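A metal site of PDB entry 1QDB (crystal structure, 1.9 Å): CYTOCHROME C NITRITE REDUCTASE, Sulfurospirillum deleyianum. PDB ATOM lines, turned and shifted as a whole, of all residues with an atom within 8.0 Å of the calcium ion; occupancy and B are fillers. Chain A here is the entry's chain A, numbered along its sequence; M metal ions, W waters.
Water W2 lies within hydrogen-bond range of the side-chain carboxylate (OD2) of Asp 226 (2.7 Å) and the side-chain hydroxyl (OH) of Tyr 219 (2.9 Å).
Water W1 lies within hydrogen-bond range of the side-chain carboxylate of Asp 226 and the side-chain amide nitrogen of Gln 240.
The calcium ion is bound by O of Lys 238 (2.5 Å), O of Tyr 176 (2.5 Å), OE1 of Gln 240 (2.5 Å), water W1 (2.6 Å), OE2 of Glu 175 (2.7 Å), water W2 (2.7 Å) and OE1 of Glu 175 (2.7 Å).
The calcium ion has seven donor atoms within binding distance.
N of Lys 238 is in hydrogen-bond range of OD2 of Asp 226, 2.9 Å away.
The side-chain carboxylate (OD2) of Asp 359 lies within salt-bridge range of the side-chain amino group (NZ) of Lys 238 (3.0 Å).
The side-chain carboxylate (OE2) of Glu 175 lies close to the side-chain hydroxyl (OH) of Tyr 219.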
ATOM      1  N   TYR A  48     -13.410 -13.775  18.031  1.00  0.00           N
ATOM      2  CA  TYR A  48     -12.488 -14.381  17.050  1.00  0.00           C
ATOM      3  C   TYR A  48     -12.601 -13.641  15.723  1.00  0.00           C
ATOM      4  O   TYR A  48     -13.586 -12.952  15.472  1.00  0.00           O
ATOM      5  CB  TYR A  48     -12.855 -15.868  16.874  1.00  0.00           C
ATOM      6  CG  TYR A  48     -11.756 -16.770  16.351  1.00  0.00           C
ATOM      7  CD1 TYR A  48     -10.530 -16.878  17.022  1.00  0.00           C
ATOM      8  CD2 TYR A  48     -11.957 -17.557  15.218  1.00  0.00           C
ATOM      9  CE1 TYR A  48      -9.541 -17.755  16.572  1.00  0.00           C
ATOM     10  CE2 TYR A  48     -10.968 -18.433  14.768  1.00  0.00           C
ATOM     11  CZ  TYR A  48      -9.771 -18.534  15.445  1.00  0.00           C
ATOM     12  OH  TYR A  48      -8.813 -19.412  15.017  1.00  0.00           O
ATOM     13  N   PHE A  50     -13.338 -14.622  12.787  1.00  0.00           N
ATOM     14  CA  PHE A  50     -14.497 -14.982  11.995  1.00  0.00           C
ATOM     15  C   PHE A  50     -15.754 -14.159  12.308  1.00  0.00           C
ATOM     16  O   PHE A  50     -16.688 -14.144  11.510  1.00  0.00           O
ATOM     17  CB  PHE A  50     -14.774 -16.485  12.087  1.00  0.00           C
ATOM     18  CG  PHE A  50     -13.822 -17.329  11.278  1.00  0.00           C
ATOM     19  CD1 PHE A  50     -12.522 -17.562  11.709  1.00  0.00           C
ATOM     20  CD2 PHE A  50     -14.246 -17.905  10.074  1.00  0.00           C
ATOM     21  CE1 PHE A  50     -11.641 -18.369  10.959  1.00  0.00           C
ATOM     22  CE2 PHE A  50     -13.364 -18.716   9.315  1.00  0.00           C
ATOM     23  CZ  PHE A  50     -12.065 -18.941   9.765  1.00  0.00           C
ATOM     24  N   VAL A 174      -9.120 -29.261   4.226  1.00  0.00           N
ATOM     25  CA  VAL A 174      -9.122 -30.077   5.429  1.00  0.00           C
ATOM     26  C   VAL A 174      -9.176 -29.165   6.667  1.00  0.00           C
ATOM     27  O   VAL A 174      -8.939 -27.949   6.571  1.00  0.00           O
ATOM     28  CB  VAL A 174      -7.823 -30.917   5.534  1.00  0.00           C
ATOM     29  CG1 VAL A 174      -7.814 -32.038   4.488  1.00  0.00           C
ATOM     30  CG2 VAL A 174      -6.600 -30.018   5.367  1.00  0.00           C
ATOM     31  N   GLU A 175      -9.534 -29.753   7.801  1.00  0.00           N
ATOM     32  CA  GLU A 175      -9.583 -29.036   9.074  1.00  0.00           C
ATOM     33  C   GLU A 175      -8.145 -29.035   9.610  1.00  0.00           C
ATOM     34  O   GLU A 175      -7.385 -29.985   9.377  1.00  0.00           O
ATOM     35  CB  GLU A 175     -10.533 -29.753  10.050  1.00  0.00           C
ATOM     36  CG  GLU A 175     -10.114 -29.764  11.522  1.00  0.00           C
ATOM     37  CD  GLU A 175     -10.187 -28.387  12.216  1.00  0.00           C
ATOM     38  OE1 GLU A 175     -10.581 -27.400  11.580  1.00  0.00           O
ATOM     39  OE2 GLU A 175      -9.810 -28.311  13.403  1.00  0.00           O
ATOM     40  N   TYR A 176      -7.762 -27.976  10.325  1.00  0.00           N
ATOM     41  CA  TYR A 176      -6.406 -27.860  10.844  1.00  0.00           C
ATOM     42  C   TYR A 176      -6.365 -26.906  12.035  1.00  0.00           C
ATOM     43  O   TYR A 176      -7.343 -26.245  12.335  1.00  0.00           O
ATOM     44  CB  TYR A 176      -5.517 -27.238   9.755  1.00  0.00           C
ATOM     45  CG  TYR A 176      -5.877 -25.788   9.483  1.00  0.00           C
ATOM     46  CD1 TYR A 176      -6.908 -25.445   8.594  1.00  0.00           C
ATOM     47  CD2 TYR A 176      -5.252 -24.744  10.190  1.00  0.00           C
ATOM     48  CE1 TYR A 176      -7.316 -24.118   8.436  1.00  0.00           C
ATOM     49  CE2 TYR A 176      -5.655 -23.424  10.035  1.00  0.00           C
ATOM     50  CZ  TYR A 176      -6.684 -23.111   9.168  1.00  0.00           C
ATOM     51  OH  TYR A 176      -7.084 -21.797   9.059  1.00  0.00           O
ATOM     52  N   TYR A 177      -5.196 -26.786  12.655  1.00  0.00           N
ATOM     53  CA  TYR A 177      -4.982 -25.834  13.744  1.00  0.00           C
ATOM     54  C   TYR A 177      -3.529 -25.393  13.649  1.00  0.00           C
ATOM     55  O   TYR A 177      -2.738 -25.975  12.902  1.00  0.00           O
ATOM     56  CB  TYR A 177      -5.309 -26.414  15.123  1.00  0.00           C
ATOM     57  CG  TYR A 177      -4.306 -27.401  15.679  1.00  0.00           C
ATOM     58  CD1 TYR A 177      -4.211 -28.703  15.182  1.00  0.00           C
ATOM     59  CD2 TYR A 177      -3.479 -27.047  16.756  1.00  0.00           C
ATOM     60  CE1 TYR A 177      -3.327 -29.623  15.739  1.00  0.00           C
ATOM     61  CE2 TYR A 177      -2.596 -27.962  17.322  1.00  0.00           C
ATOM     62  CZ  TYR A 177      -2.518 -29.246  16.806  1.00  0.00           C
ATOM     63  OH  TYR A 177      -1.649 -30.156  17.381  1.00  0.00           O
ATOM     64  N   PHE A 178      -3.199 -24.316  14.345  1.00  0.00           N
ATOM     65  CA  PHE A 178      -1.824 -23.817  14.343  1.00  0.00           C
ATOM     66  C   PHE A 178      -1.145 -24.349  15.590  1.00  0.00           C
ATOM     67  O   PHE A 178      -1.555 -24.047  16.709  1.00  0.00           O
ATOM     68  CB  PHE A 178      -1.805 -22.293  14.365  1.00  0.00           C
ATOM     69  CG  PHE A 178      -2.348 -21.653  13.121  1.00  0.00           C
ATOM     70  CD1 PHE A 178      -2.425 -22.355  11.925  1.00  0.00           C
ATOM     71  CD2 PHE A 178      -2.772 -20.327  13.146  1.00  0.00           C
ATOM     72  CE1 PHE A 178      -2.917 -21.757  10.774  1.00  0.00           C
ATOM     73  CE2 PHE A 178      -3.270 -19.721  11.992  1.00  0.00           C
ATOM     74  CZ  PHE A 178      -3.349 -20.433  10.811  1.00  0.00           C
ATOM     75  N   THR A 197      -1.289 -27.782  11.309  1.00  0.00           N
ATOM     76  CA  THR A 197      -1.333 -29.169  11.716  1.00  0.00           C
ATOM     77  C   THR A 197      -2.745 -29.748  11.599  1.00  0.00           C
ATOM     78  O   THR A 197      -3.712 -29.128  12.034  1.00  0.00           O
ATOM     79  CB  THR A 197      -0.873 -29.297  13.183  1.00  0.00           C
ATOM     80  OG1 THR A 197       0.386 -28.657  13.348  1.00  0.00           O
ATOM     81  CG2 THR A 197      -0.742 -30.757  13.603  1.00  0.00           C
ATOM     82  N   PRO A 199      -5.400 -32.265  12.865  1.00  0.00           N
ATOM     83  CA  PRO A 199      -5.688 -33.008  14.106  1.00  0.00           C
ATOM     84  C   PRO A 199      -6.267 -34.387  13.817  1.00  0.00           C
ATOM     85  O   PRO A 199      -7.330 -34.758  14.336  1.00  0.00           O
ATOM     86  CB  PRO A 199      -6.686 -32.101  14.803  1.00  0.00           C
ATOM     87  CG  PRO A 199      -7.501 -31.557  13.644  1.00  0.00           C
ATOM     88  CD  PRO A 199      -6.453 -31.271  12.576  1.00  0.00           C
ATOM     89  N   MET A 215     -11.323 -35.843  16.963  1.00  0.00           N
ATOM     90  CA  MET A 215     -10.656 -34.540  17.005  1.00  0.00           C
ATOM     91  C   MET A 215     -10.882 -33.862  18.354  1.00  0.00           C
ATOM     92  O   MET A 215      -9.952 -33.277  18.931  1.00  0.00           O
ATOM     93  CB  MET A 215     -11.156 -33.632  15.870  1.00  0.00           C
ATOM     94  CG  MET A 215     -10.580 -33.981  14.494  1.00  0.00           C
ATOM     95  SD  MET A 215     -11.333 -32.975  13.205  1.00  0.00           S
ATOM     96  CE  MET A 215     -10.845 -33.824  11.695  1.00  0.00           C
ATOM     97  N   TYR A 219      -7.941 -32.622  20.739  1.00  0.00           N
ATOM     98  CA  TYR A 219      -7.803 -31.235  21.164  1.00  0.00           C
ATOM     99  C   TYR A 219      -7.878 -31.061  22.689  1.00  0.00           C
ATOM    100  O   TYR A 219      -7.113 -30.279  23.246  1.00  0.00           O
ATOM    101  CB  TYR A 219      -8.845 -30.348  20.476  1.00  0.00           C
ATOM    102  CG  TYR A 219      -8.520 -30.022  19.037  1.00  0.00           C
ATOM    103  CD1 TYR A 219      -7.274 -29.476  18.689  1.00  0.00           C
ATOM    104  CD2 TYR A 219      -9.479 -30.156  18.030  1.00  0.00           C
ATOM    105  CE1 TYR A 219      -7.015 -29.083  17.373  1.00  0.00           C
ATOM    106  CE2 TYR A 219      -9.222 -29.772  16.727  1.00  0.00           C
ATOM    107  CZ  TYR A 219      -7.993 -29.226  16.411  1.00  0.00           C
ATOM    108  OH  TYR A 219      -7.758 -28.788  15.119  1.00  0.00           O
ATOM    109  N   PHE A 224      -5.825 -27.707  23.840  1.00  0.00           N
ATOM    110  CA  PHE A 224      -5.727 -26.620  22.875  1.00  0.00           C
ATOM    111  C   PHE A 224      -7.047 -25.898  22.656  1.00  0.00           C
ATOM    112  O   PHE A 224      -8.109 -26.502  22.687  1.00  0.00           O
ATOM    113  CB  PHE A 224      -5.204 -27.168  21.536  1.00  0.00           C
ATOM    114  CG  PHE A 224      -5.174 -26.141  20.432  1.00  0.00           C
ATOM    115  CD1 PHE A 224      -4.082 -25.296  20.283  1.00  0.00           C
ATOM    116  CD2 PHE A 224      -6.275 -25.965  19.597  1.00  0.00           C
ATOM    117  CE1 PHE A 224      -4.088 -24.292  19.316  1.00  0.00           C
ATOM    118  CE2 PHE A 224      -6.290 -24.967  18.633  1.00  0.00           C
ATOM    119  CZ  PHE A 224      -5.192 -24.129  18.487  1.00  0.00           C
ATOM    120  N   ASP A 226      -8.596 -22.459  20.179  1.00  0.00           N
ATOM    121  CA  ASP A 226      -8.312 -21.465  19.160  1.00  0.00           C
ATOM    122  C   ASP A 226      -8.515 -20.063  19.743  1.00  0.00           C
ATOM    123  O   ASP A 226      -7.852 -19.123  19.317  1.00  0.00           O
ATOM    124  CB  ASP A 226      -9.191 -21.669  17.935  1.00  0.00           C
ATOM    125  CG  ASP A 226      -8.813 -22.907  17.161  1.00  0.00           C
ATOM    126  OD1 ASP A 226      -7.820 -22.828  16.401  1.00  0.00           O
ATOM    127  OD2 ASP A 226      -9.483 -23.947  17.336  1.00  0.00           O
ATOM    128  N   LEU A 237     -13.055 -24.071  20.060  1.00  0.00           N
ATOM    129  CA  LEU A 237     -12.402 -24.735  18.933  1.00  0.00           C
ATOM    130  C   LEU A 237     -13.059 -24.269  17.648  1.00  0.00           C
ATOM    131  O   LEU A 237     -14.287 -24.356  17.531  1.00  0.00           O
ATOM    132  CB  LEU A 237     -12.531 -26.260  19.017  1.00  0.00           C
ATOM    133  CG  LEU A 237     -11.801 -26.958  20.159  1.00  0.00           C
ATOM    134  CD1 LEU A 237     -12.152 -28.420  20.168  1.00  0.00           C
ATOM    135  CD2 LEU A 237     -10.298 -26.755  20.011  1.00  0.00           C
ATOM    136  N   LYS A 238     -12.272 -23.773  16.704  1.00  0.00           N
ATOM    137  CA  LYS A 238     -12.815 -23.306  15.432  1.00  0.00           C
ATOM    138  C   LYS A 238     -12.685 -24.417  14.406  1.00  0.00           C
ATOM    139  O   LYS A 238     -11.659 -25.062  14.339  1.00  0.00           O
ATOM    140  CB  LYS A 238     -12.021 -22.101  14.914  1.00  0.00           C
ATOM    141  CG  LYS A 238     -12.512 -21.553  13.579  1.00  0.00           C
ATOM    142  CD  LYS A 238     -13.845 -20.802  13.736  1.00  0.00           C
ATOM    143  CE  LYS A 238     -14.445 -20.428  12.382  1.00  0.00           C
ATOM    144  NZ  LYS A 238     -15.198 -21.547  11.702  1.00  0.00           N
ATOM    145  N   ALA A 239     -13.712 -24.615  13.595  1.00  0.00           N
ATOM    146  CA  ALA A 239     -13.652 -25.624  12.559  1.00  0.00           C
ATOM    147  C   ALA A 239     -13.356 -24.923  11.238  1.00  0.00           C
ATOM    148  O   ALA A 239     -13.794 -23.793  11.018  1.00  0.00           O
ATOM    149  CB  ALA A 239     -14.966 -26.358  12.463  1.00  0.00           C
ATOM    150  N   GLN A 240     -12.600 -25.572  10.366  1.00  0.00           N
ATOM    151  CA  GLN A 240     -12.329 -24.995   9.051  1.00  0.00           C
ATOM    152  C   GLN A 240     -12.420 -26.039   7.960  1.00  0.00           C
ATOM    153  O   GLN A 240     -11.762 -27.075   8.029  1.00  0.00           O
ATOM    154  CB  GLN A 240     -10.940 -24.349   8.958  1.00  0.00           C
ATOM    155  CG  GLN A 240     -10.820 -22.969   9.591  1.00  0.00           C
ATOM    156  CD  GLN A 240     -10.145 -23.024  10.926  1.00  0.00           C
ATOM    157  OE1 GLN A 240      -9.926 -24.098  11.462  1.00  0.00           O
ATOM    158  NE2 GLN A 240      -9.799 -21.861  11.480  1.00  0.00           N
ATOM    159  N   HIS A 241     -13.297 -25.765   7.005  1.00  0.00           N
ATOM    160  CA  HIS A 241     -13.497 -26.578   5.807  1.00  0.00           C
ATOM    161  C   HIS A 241     -12.933 -28.003   5.826  1.00  0.00           C
ATOM    162  O   HIS A 241     -11.909 -28.288   5.192  1.00  0.00           O
ATOM    163  CB  HIS A 241     -12.902 -25.814   4.619  1.00  0.00           C
ATOM    164  CG  HIS A 241     -11.590 -25.159   4.941  1.00  0.00           C
ATOM    165  ND1 HIS A 241     -10.466 -25.871   5.292  1.00  0.00           N
ATOM    166  CD2 HIS A 241     -11.257 -23.841   5.066  1.00  0.00           C
ATOM    167  CE1 HIS A 241      -9.495 -25.035   5.628  1.00  0.00           C
ATOM    168  NE2 HIS A 241      -9.955 -23.804   5.496  1.00  0.00           N
ATOM    169  N   PHE A 356     -18.220 -27.080  18.145  1.00  0.00           N
ATOM    170  CA  PHE A 356     -17.223 -27.657  17.251  1.00  0.00           C
ATOM    171  C   PHE A 356     -17.900 -28.651  16.318  1.00  0.00           C
ATOM    172  O   PHE A 356     -17.655 -28.649  15.115  1.00  0.00           O
ATOM    173  CB  PHE A 356     -16.077 -28.327  18.006  1.00  0.00           C
ATOM    174  CG  PHE A 356     -14.942 -28.799  17.106  1.00  0.00           C
ATOM    175  CD1 PHE A 356     -14.186 -27.883  16.390  1.00  0.00           C
ATOM    176  CD2 PHE A 356     -14.657 -30.159  16.972  1.00  0.00           C
ATOM    177  CE1 PHE A 356     -13.151 -28.326  15.518  1.00  0.00           C
ATOM    178  CE2 PHE A 356     -13.644 -30.603  16.111  1.00  0.00           C
ATOM    179  CZ  PHE A 356     -12.886 -29.673  15.390  1.00  0.00           C
ATOM    180  N   ASP A 359     -20.035 -26.627  13.921  1.00  0.00           N
ATOM    181  CA  ASP A 359     -19.175 -25.836  13.032  1.00  0.00           C
ATOM    182  C   ASP A 359     -18.506 -26.752  11.975  1.00  0.00           C
ATOM    183  O   ASP A 359     -18.447 -26.429  10.800  1.00  0.00           O
ATOM    184  CB  ASP A 359     -18.118 -25.109  13.868  1.00  0.00           C
ATOM    185  CG  ASP A 359     -17.474 -23.927  13.129  1.00  0.00           C
ATOM    186  OD1 ASP A 359     -17.905 -23.589  12.009  1.00  0.00           O
ATOM    187  OD2 ASP A 359     -16.528 -23.336  13.692  1.00  0.00           O
ATOM    188  N   MET A 360     -18.003 -27.897  12.418  1.00  0.00           N
ATOM    189  CA  MET A 360     -17.392 -28.844  11.491  1.00  0.00           C
ATOM    190  C   MET A 360     -18.402 -29.240  10.404  1.00  0.00           C
ATOM    191  O   MET A 360     -18.066 -29.291   9.225  1.00  0.00           O
ATOM    192  CB  MET A 360     -16.893 -30.089  12.244  1.00  0.00           C
ATOM    193  CG  MET A 360     -15.579 -29.884  12.985  1.00  0.00           C
ATOM    194  SD  MET A 360     -14.193 -29.633  11.843  1.00  0.00           S
ATOM    195  CE  MET A 360     -13.799 -31.342  11.443  1.00  0.00           C
HETATM  196 CA    CA M   1      -9.516 -25.668  13.315  1.00  0.00          CA
HETATM  197  O   HOH W   1      -8.329 -23.386  13.851  1.00  0.00           O
HETATM  198  O   HOH W   2      -8.894 -26.188  15.861  1.00  0.00           O
